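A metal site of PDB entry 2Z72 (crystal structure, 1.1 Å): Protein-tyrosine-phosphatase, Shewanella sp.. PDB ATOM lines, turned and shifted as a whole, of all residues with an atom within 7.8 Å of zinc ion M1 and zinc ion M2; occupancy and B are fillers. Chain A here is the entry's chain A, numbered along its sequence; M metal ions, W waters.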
ATOM      1  N   SER A  77      -3.482   3.941  11.988  1.00  0.00           N
ATOM      2  CA  SER A  77      -3.132   2.855  12.903  1.00  0.00           C
ATOM      3  C   SER A  77      -2.072   3.276  13.888  1.00  0.00           C
ATOM      4  O   SER A  77      -1.387   4.275  13.728  1.00  0.00           O
ATOM      5  CB  SER A  77      -2.531   1.733  12.066  1.00  0.00           C
ATOM      6  OG  SER A  77      -2.548   0.497  12.753  1.00  0.00           O
ATOM      7  N   ASP A  78      -1.920   2.482  14.927  1.00  0.00           N
ATOM      8  CA  ASP A  78      -0.778   2.533  15.846  1.00  0.00           C
ATOM      9  C   ASP A  78      -0.621   3.907  16.488  1.00  0.00           C
ATOM     10  O   ASP A  78       0.449   4.492  16.591  1.00  0.00           O
ATOM     11  CB  ASP A  78       0.511   2.108  15.123  1.00  0.00           C
ATOM     12  CG  ASP A  78       0.483   0.636  14.741  1.00  0.00           C
ATOM     13  OD1 ASP A  78       0.932  -0.241  15.500  1.00  0.00           O
ATOM     14  OD2 ASP A  78      -0.093   0.347  13.643  1.00  0.00           O
ATOM     15  N   VAL A  79      -1.760   4.419  17.008  1.00  0.00           N
ATOM     16  CA  VAL A  79      -1.707   5.689  17.726  1.00  0.00           C
ATOM     17  C   VAL A  79      -0.867   5.579  19.012  1.00  0.00           C
ATOM     18  O   VAL A  79      -0.246   6.558  19.388  1.00  0.00           O
ATOM     19  CB  VAL A  79      -3.159   6.152  17.984  1.00  0.00           C
ATOM     20  CG1 VAL A  79      -3.227   7.322  18.936  1.00  0.00           C
ATOM     21  CG2 VAL A  79      -3.868   6.479  16.677  1.00  0.00           C
ATOM     22  N   HIS A  80      -0.902   4.425  19.681  1.00  0.00           N
ATOM     23  CA  HIS A  80      -0.008   4.192  20.826  1.00  0.00           C
ATOM     24  C   HIS A  80      -0.067   5.328  21.823  1.00  0.00           C
ATOM     25  O   HIS A  80       0.920   5.946  22.213  1.00  0.00           O
ATOM     26  CB  HIS A  80       1.433   3.911  20.339  1.00  0.00           C
ATOM     27  CG  HIS A  80       1.552   2.512  19.819  1.00  0.00           C
ATOM     28  ND1 HIS A  80       1.271   1.417  20.583  1.00  0.00           N
ATOM     29  CD2 HIS A  80       1.970   2.018  18.624  1.00  0.00           C
ATOM     30  CE1 HIS A  80       1.465   0.326  19.872  1.00  0.00           C
ATOM     31  NE2 HIS A  80       1.905   0.629  18.640  1.00  0.00           N
ATOM     32  N   THR A 112      -6.588   0.351  12.385  1.00  0.00           N
ATOM     33  CA  THR A 112      -6.112  -1.031  12.391  1.00  0.00           C
ATOM     34  C   THR A 112      -5.284  -1.392  13.608  1.00  0.00           C
ATOM     35  O   THR A 112      -4.222  -2.033  13.468  1.00  0.00           O
ATOM     36  CB  THR A 112      -5.359  -1.369  11.097  1.00  0.00           C
ATOM     37  OG1 THR A 112      -4.282  -0.489  10.914  1.00  0.00           O
ATOM     38  CG2 THR A 112      -6.264  -1.186   9.851  1.00  0.00           C
ATOM     39  N   GLY A 113      -5.756  -1.029  14.812  1.00  0.00           N
ATOM     40  CA  GLY A 113      -5.141  -1.503  16.048  1.00  0.00           C
ATOM     41  C   GLY A 113      -4.111  -0.582  16.682  1.00  0.00           C
ATOM     42  O   GLY A 113      -3.709   0.444  16.168  1.00  0.00           O
ATOM     43  N   ASP A 114      -3.733  -1.002  17.884  1.00  0.00           N
ATOM     44  CA  ASP A 114      -2.620  -0.412  18.667  1.00  0.00           C
ATOM     45  C   ASP A 114      -2.857   1.002  19.099  1.00  0.00           C
ATOM     46  O   ASP A 114      -2.036   1.905  18.986  1.00  0.00           O
ATOM     47  CB  ASP A 114      -1.282  -0.585  17.951  1.00  0.00           C
ATOM     48  CG  ASP A 114      -0.640  -1.929  18.165  1.00  0.00           C
ATOM     49  OD1 ASP A 114       0.609  -2.032  17.757  1.00  0.00           O
ATOM     50  OD2 ASP A 114      -1.285  -2.864  18.666  1.00  0.00           O
ATOM     51  N   ILE A 115      -4.039   1.192  19.745  1.00  0.00           N
ATOM     52  CA  ILE A 115      -4.283   2.349  20.597  1.00  0.00           C
ATOM     53  C   ILE A 115      -3.420   2.297  21.848  1.00  0.00           C
ATOM     54  O   ILE A 115      -2.828   3.279  22.281  1.00  0.00           O
ATOM     55  CB  ILE A 115      -5.764   2.454  20.993  1.00  0.00           C
ATOM     56  CG1 ILE A 115      -6.606   2.855  19.787  1.00  0.00           C
ATOM     57  CG2 ILE A 115      -5.928   3.417  22.168  1.00  0.00           C
ATOM     58  CD1 ILE A 115      -8.102   2.834  20.011  1.00  0.00           C
ATOM     59  N   PHE A 116      -3.384   1.123  22.486  1.00  0.00           N
ATOM     60  CA  PHE A 116      -2.644   0.966  23.741  1.00  0.00           C
ATOM     61  C   PHE A 116      -1.125   1.047  23.562  1.00  0.00           C
ATOM     62  O   PHE A 116      -0.585   0.756  22.507  1.00  0.00           O
ATOM     63  CB  PHE A 116      -2.951  -0.366  24.364  1.00  0.00           C
ATOM     64  CG  PHE A 116      -4.319  -0.485  24.989  1.00  0.00           C
ATOM     65  CD1 PHE A 116      -5.403  -1.004  24.290  1.00  0.00           C
ATOM     66  CD2 PHE A 116      -4.505  -0.072  26.290  1.00  0.00           C
ATOM     67  CE1 PHE A 116      -6.621  -1.098  24.902  1.00  0.00           C
ATOM     68  CE2 PHE A 116      -5.726  -0.174  26.871  1.00  0.00           C
ATOM     69  CZ  PHE A 116      -6.780  -0.702  26.212  1.00  0.00           C
ATOM     70  N   ASP A 117      -0.504   1.417  24.676  1.00  0.00           N
ATOM     71  CA  ASP A 117       0.904   1.263  25.020  1.00  0.00           C
ATOM     72  C   ASP A 117       1.786   2.347  24.404  1.00  0.00           C
ATOM     73  O   ASP A 117       1.438   3.025  23.449  1.00  0.00           O
ATOM     74  CB  ASP A 117       1.384  -0.146  24.663  1.00  0.00           C
ATOM     75  CG  ASP A 117       0.814  -1.228  25.560  1.00  0.00           C
ATOM     76  OD1 ASP A 117       1.015  -2.431  25.212  1.00  0.00           O
ATOM     77  OD2 ASP A 117       0.216  -0.892  26.606  1.00  0.00           O
ATOM     78  N   GLY A 148      -5.346  -4.755  17.650  1.00  0.00           N
ATOM     79  CA  GLY A 148      -3.951  -4.972  17.351  1.00  0.00           C
ATOM     80  C   GLY A 148      -3.280  -5.828  18.351  1.00  0.00           C
ATOM     81  O   GLY A 148      -3.881  -6.320  19.335  1.00  0.00           O
ATOM     82  N   ASN A 149      -1.958  -6.058  18.191  1.00  0.00           N
ATOM     83  CA  ASN A 149      -1.271  -6.884  19.159  1.00  0.00           C
ATOM     84  C   ASN A 149      -1.243  -6.242  20.541  1.00  0.00           C
ATOM     85  O   ASN A 149      -1.320  -7.005  21.518  1.00  0.00           O
ATOM     86  CB  ASN A 149       0.155  -7.281  18.694  1.00  0.00           C
ATOM     87  CG  ASN A 149       1.102  -6.160  18.515  1.00  0.00           C
ATOM     88  OD1 ASN A 149       0.785  -5.164  17.859  1.00  0.00           O
ATOM     89  ND2 ASN A 149       2.328  -6.268  18.981  1.00  0.00           N
ATOM     90  N   HIS A 150      -1.173  -4.917  20.621  1.00  0.00           N
ATOM     91  CA  HIS A 150      -1.177  -4.336  21.984  1.00  0.00           C
ATOM     92  C   HIS A 150      -2.521  -4.395  22.654  1.00  0.00           C
ATOM     93  O   HIS A 150      -2.574  -4.536  23.893  1.00  0.00           O
ATOM     94  CB  HIS A 150      -0.613  -2.932  21.960  1.00  0.00           C
ATOM     95  CG  HIS A 150       0.886  -2.981  21.742  1.00  0.00           C
ATOM     96  ND1 HIS A 150       1.770  -2.847  22.798  1.00  0.00           N
ATOM     97  CD2 HIS A 150       1.587  -3.188  20.621  1.00  0.00           C
ATOM     98  CE1 HIS A 150       2.965  -2.968  22.291  1.00  0.00           C
ATOM     99  NE2 HIS A 150       2.939  -3.171  20.981  1.00  0.00           N
ATOM    100  N   GLU A 151      -3.652  -4.325  21.957  1.00  0.00           N
ATOM    101  CA  GLU A 151      -4.939  -4.608  22.587  1.00  0.00           C
ATOM    102  C   GLU A 151      -4.954  -6.005  23.181  1.00  0.00           C
ATOM    103  O   GLU A 151      -5.426  -6.231  24.287  1.00  0.00           O
ATOM    104  CB  GLU A 151      -6.109  -4.417  21.630  1.00  0.00           C
ATOM    105  CG  GLU A 151      -6.477  -2.997  21.296  1.00  0.00           C
ATOM    106  CD  GLU A 151      -5.403  -2.244  20.553  1.00  0.00           C
ATOM    107  OE1 GLU A 151      -5.103  -1.096  20.900  1.00  0.00           O
ATOM    108  OE2 GLU A 151      -4.891  -2.843  19.577  1.00  0.00           O
ATOM    109  N   MET A 153      -2.381  -7.922  24.008  1.00  0.00           N
ATOM    110  CA  MET A 153      -1.418  -8.018  25.111  1.00  0.00           C
ATOM    111  C   MET A 153      -2.014  -7.432  26.394  1.00  0.00           C
ATOM    112  O   MET A 153      -2.053  -8.074  27.430  1.00  0.00           O
ATOM    113  CB  MET A 153      -0.117  -7.311  24.763  1.00  0.00           C
ATOM    114  CG  MET A 153       0.791  -8.310  24.017  1.00  0.00           C
ATOM    115  SD  MET A 153       2.470  -7.723  23.829  1.00  0.00           S
ATOM    116  CE  MET A 153       2.323  -6.465  22.581  1.00  0.00           C
ATOM    117  N   HIS A 207      -4.089  -5.649  11.506  1.00  0.00           N
ATOM    118  CA  HIS A 207      -2.980  -4.957  12.128  1.00  0.00           C
ATOM    119  C   HIS A 207      -1.614  -5.305  11.550  1.00  0.00           C
ATOM    120  O   HIS A 207      -0.842  -4.403  11.199  1.00  0.00           O
ATOM    121  CB  HIS A 207      -3.026  -5.228  13.632  1.00  0.00           C
ATOM    122  CG  HIS A 207      -1.955  -4.481  14.362  1.00  0.00           C
ATOM    123  ND1 HIS A 207      -1.980  -3.103  14.422  1.00  0.00           N
ATOM    124  CD2 HIS A 207      -0.857  -4.872  15.018  1.00  0.00           C
ATOM    125  CE1 HIS A 207      -0.923  -2.696  15.065  1.00  0.00           C
ATOM    126  NE2 HIS A 207      -0.182  -3.744  15.480  1.00  0.00           N
ATOM    127  N   GLY A 208      -1.280  -6.578  11.470  1.00  0.00           N
ATOM    128  CA  GLY A 208       0.043  -7.054  11.082  1.00  0.00           C
ATOM    129  C   GLY A 208       0.134  -7.458   9.641  1.00  0.00           C
ATOM    130  O   GLY A 208       0.866  -6.886   8.824  1.00  0.00           O
ATOM    131  N   THR A 255      -2.087 -10.379  13.804  1.00  0.00           N
ATOM    132  CA  THR A 255      -1.768  -9.189  14.580  1.00  0.00           C
ATOM    133  C   THR A 255      -0.293  -8.991  14.880  1.00  0.00           C
ATOM    134  O   THR A 255       0.078  -7.928  15.365  1.00  0.00           O
ATOM    135  CB  THR A 255      -2.555  -9.150  15.892  1.00  0.00           C
ATOM    136  OG1 THR A 255      -2.235 -10.324  16.625  1.00  0.00           O
ATOM    137  CG2 THR A 255      -4.043  -9.072  15.625  1.00  0.00           C
ATOM    138  N   TRP A 256       0.564  -9.926  14.475  1.00  0.00           N
ATOM    139  CA  TRP A 256       2.011  -9.778  14.669  1.00  0.00           C
ATOM    140  C   TRP A 256       2.807  -9.900  13.401  1.00  0.00           C
ATOM    141  O   TRP A 256       3.971  -9.483  13.367  1.00  0.00           O
ATOM    142  CB  TRP A 256       2.527 -10.825  15.652  1.00  0.00           C
ATOM    143  CG  TRP A 256       2.202 -10.604  17.082  1.00  0.00           C
ATOM    144  CD1 TRP A 256       1.069 -10.995  17.757  1.00  0.00           C
ATOM    145  CD2 TRP A 256       2.997  -9.928  18.036  1.00  0.00           C
ATOM    146  NE1 TRP A 256       1.122 -10.628  19.065  1.00  0.00           N
ATOM    147  CE2 TRP A 256       2.300  -9.952  19.271  1.00  0.00           C
ATOM    148  CE3 TRP A 256       4.236  -9.311  18.023  1.00  0.00           C
ATOM    149  CZ2 TRP A 256       2.814  -9.388  20.446  1.00  0.00           C
ATOM    150  CZ3 TRP A 256       4.731  -8.754  19.162  1.00  0.00           C
ATOM    151  CH2 TRP A 256       4.029  -8.773  20.373  1.00  0.00           C
ATOM    152  N   ARG A 258       4.955  -9.651  10.261  1.00  0.00           N
ATOM    153  CA  ARG A 258       5.659  -8.566   9.635  1.00  0.00           C
ATOM    154  C   ARG A 258       6.267  -8.925   8.280  1.00  0.00           C
ATOM    155  O   ARG A 258       7.110  -8.215   7.754  1.00  0.00           O
ATOM    156  CB  ARG A 258       6.808  -7.974  10.496  1.00  0.00           C
ATOM    157  CG  ARG A 258       6.242  -7.362  11.744  1.00  0.00           C
ATOM    158  CD  ARG A 258       7.315  -6.523  12.374  1.00  0.00           C
ATOM    159  NE  ARG A 258       7.046  -6.193  13.722  1.00  0.00           N
ATOM    160  CZ  ARG A 258       6.576  -5.201  14.366  1.00  0.00           C
ATOM    161  NH1 ARG A 258       6.382  -4.972  15.682  1.00  0.00           N
ATOM    162  NH2 ARG A 258       6.179  -4.165  13.620  1.00  0.00           N
ATOM    163  N   GLY A 285      -1.035  -2.026   9.657  1.00  0.00           N
ATOM    164  CA  GLY A 285      -0.282  -1.165  10.581  1.00  0.00           C
ATOM    165  C   GLY A 285       0.944  -1.899  11.081  1.00  0.00           C
ATOM    166  O   GLY A 285       1.664  -2.540  10.250  1.00  0.00           O
ATOM    167  N   HIS A 286       1.205  -1.843  12.386  1.00  0.00           N
ATOM    168  CA  HIS A 286       2.101  -2.621  13.190  1.00  0.00           C
ATOM    169  C   HIS A 286       3.578  -2.364  12.996  1.00  0.00           C
ATOM    170  O   HIS A 286       4.317  -2.326  13.989  1.00  0.00           O
ATOM    171  CB  HIS A 286       1.809  -4.131  13.036  1.00  0.00           C
ATOM    172  CG  HIS A 286       2.560  -5.066  13.910  1.00  0.00           C
ATOM    173  ND1 HIS A 286       2.577  -5.089  15.277  1.00  0.00           N
ATOM    174  CD2 HIS A 286       3.342  -6.128  13.545  1.00  0.00           C
ATOM    175  CE1 HIS A 286       3.346  -6.078  15.644  1.00  0.00           C
ATOM    176  NE2 HIS A 286       3.844  -6.766  14.631  1.00  0.00           N
ATOM    177  N   THR A 287       4.035  -2.290  11.777  1.00  0.00           N
ATOM    178  CA  THR A 287       5.405  -2.068  11.386  1.00  0.00           C
ATOM    179  C   THR A 287       5.564  -0.606  10.950  1.00  0.00           C
ATOM    180  O   THR A 287       5.096  -0.222   9.882  1.00  0.00           O
ATOM    181  CB  THR A 287       5.839  -3.067  10.293  1.00  0.00           C
ATOM    182  OG1 THR A 287       5.541  -4.393  10.713  1.00  0.00           O
ATOM    183  CG2 THR A 287       7.369  -2.949  10.082  1.00  0.00           C
ATOM    184  N   SER A 288       6.225   0.187  11.836  1.00  0.00           N
ATOM    185  CA  SER A 288       6.141   1.628  11.716  1.00  0.00           C
ATOM    186  C   SER A 288       6.973   2.141  10.536  1.00  0.00           C
ATOM    187  O   SER A 288       8.134   1.781  10.383  1.00  0.00           O
ATOM    188  CB  SER A 288       6.608   2.301  12.990  1.00  0.00           C
ATOM    189  OG  SER A 288       5.927   1.732  14.111  1.00  0.00           O
ATOM    190  N   ASP A 304       0.874   2.414   9.512  1.00  0.00           N
ATOM    191  CA  ASP A 304       1.538   2.846  10.744  1.00  0.00           C
ATOM    192  C   ASP A 304       2.523   3.921  10.302  1.00  0.00           C
ATOM    193  O   ASP A 304       3.566   3.566   9.727  1.00  0.00           O
ATOM    194  CB  ASP A 304       2.166   1.708  11.478  1.00  0.00           C
ATOM    195  CG  ASP A 304       2.901   2.134  12.754  1.00  0.00           C
ATOM    196  OD1 ASP A 304       3.302   1.221  13.490  1.00  0.00           O
ATOM    197  OD2 ASP A 304       3.029   3.377  12.976  1.00  0.00           O
ATOM    198  N   LYS A 308       3.288   6.926  17.050  1.00  0.00           N
ATOM    199  CA  LYS A 308       3.796   6.564  18.360  1.00  0.00           C
ATOM    200  C   LYS A 308       4.933   7.450  18.804  1.00  0.00           C
ATOM    201  O   LYS A 308       5.158   7.558  19.995  1.00  0.00           O
ATOM    202  CB  LYS A 308       4.256   5.103  18.396  1.00  0.00           C
ATOM    203  CG  LYS A 308       5.539   4.840  17.579  1.00  0.00           C
ATOM    204  CD  LYS A 308       5.876   3.409  17.429  1.00  0.00           C
ATOM    205  CE  LYS A 308       7.181   3.209  16.681  1.00  0.00           C
ATOM    206  NZ  LYS A 308       7.547   1.799  16.533  1.00  0.00           N
HETATM  207 ZN    ZN M   1       2.096  -0.605  17.073  1.00  0.00          ZN
HETATM  208 ZN    ZN M   2       1.518  -3.745  16.548  1.00  0.00          ZN
HETATM  209  O   HOH W   1       3.651   0.526  16.179  1.00  0.00           O
HETATM  210  O   HOH W   2       4.189  -3.986  18.629  1.00  0.00           O
HETATM  211  O   HOH W   3       2.898  -2.362  16.696  1.00  0.00           O
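OD2 of Asp 78 sits at hydrogen-bond distance from N of His 286, at 2.8 Å. The side-chain carboxylate of Asp 78 sits at hydrogen-bond distance from the side-chain hydroxyl of Ser 77 (2.6 Å). ND1 of His 80 is in hydrogen-bond range of O of Phe 116, 2.8 Å away. O of Ile 115 sits close to N of His 80, 3.4 Å away. The backbone carbonyl oxygen (O) of His 207 is in hydrogen-bond range of the backbone NH (N) of Gly 285 (2.8 Å). A ring nitrogen (NE2) of His 286 is in hydrogen-bond range of the backbone carbonyl oxygen of Trp 256, at 3.0 Å. The backbone carbonyl oxygen (O) of Asp 114 lies within hydrogen-bond range of the backbone NH (N) of Val 79 (3.2 Å). N of Asp 114 is in hydrogen-bond range of OE2 of Glu 151.
The nearest printed residue that does not touch zinc ion M1 is His 286 (4.2 Å).
Of the 26 residues printed, 5 come within 4 Å of zinc ion M2. The nearest printed residue that does not touch zinc ion M2 is His 150 (4.1 Å).
Zinc ion M1 is bound by water W3 (2.0 Å), OD1 of Asp 78 (2.0 Å), NE2 of His 80 (2.0 Å), water W1 (2.1 Å) and OD1 of Asp 114 (2.2 Å).
Zinc ion M2 is bound by water W3 (2.0 Å), a ring nitrogen (NE2) of His 207 (2.0 Å), the side-chain amide oxygen of Asn 149 (2.1 Å), a ring nitrogen (ND1) of His 286 (2.1 Å) and the side-chain carboxylate of Asp 114 (2.3 Å). Zinc ion M2 has five donor atoms within binding distance.
Water W1 lies within hydrogen-bond range of OD1 of Asp 304 and OG of Ser 288. Water W2 bridges NE2 of His 150 and ND2 of Asn 149.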
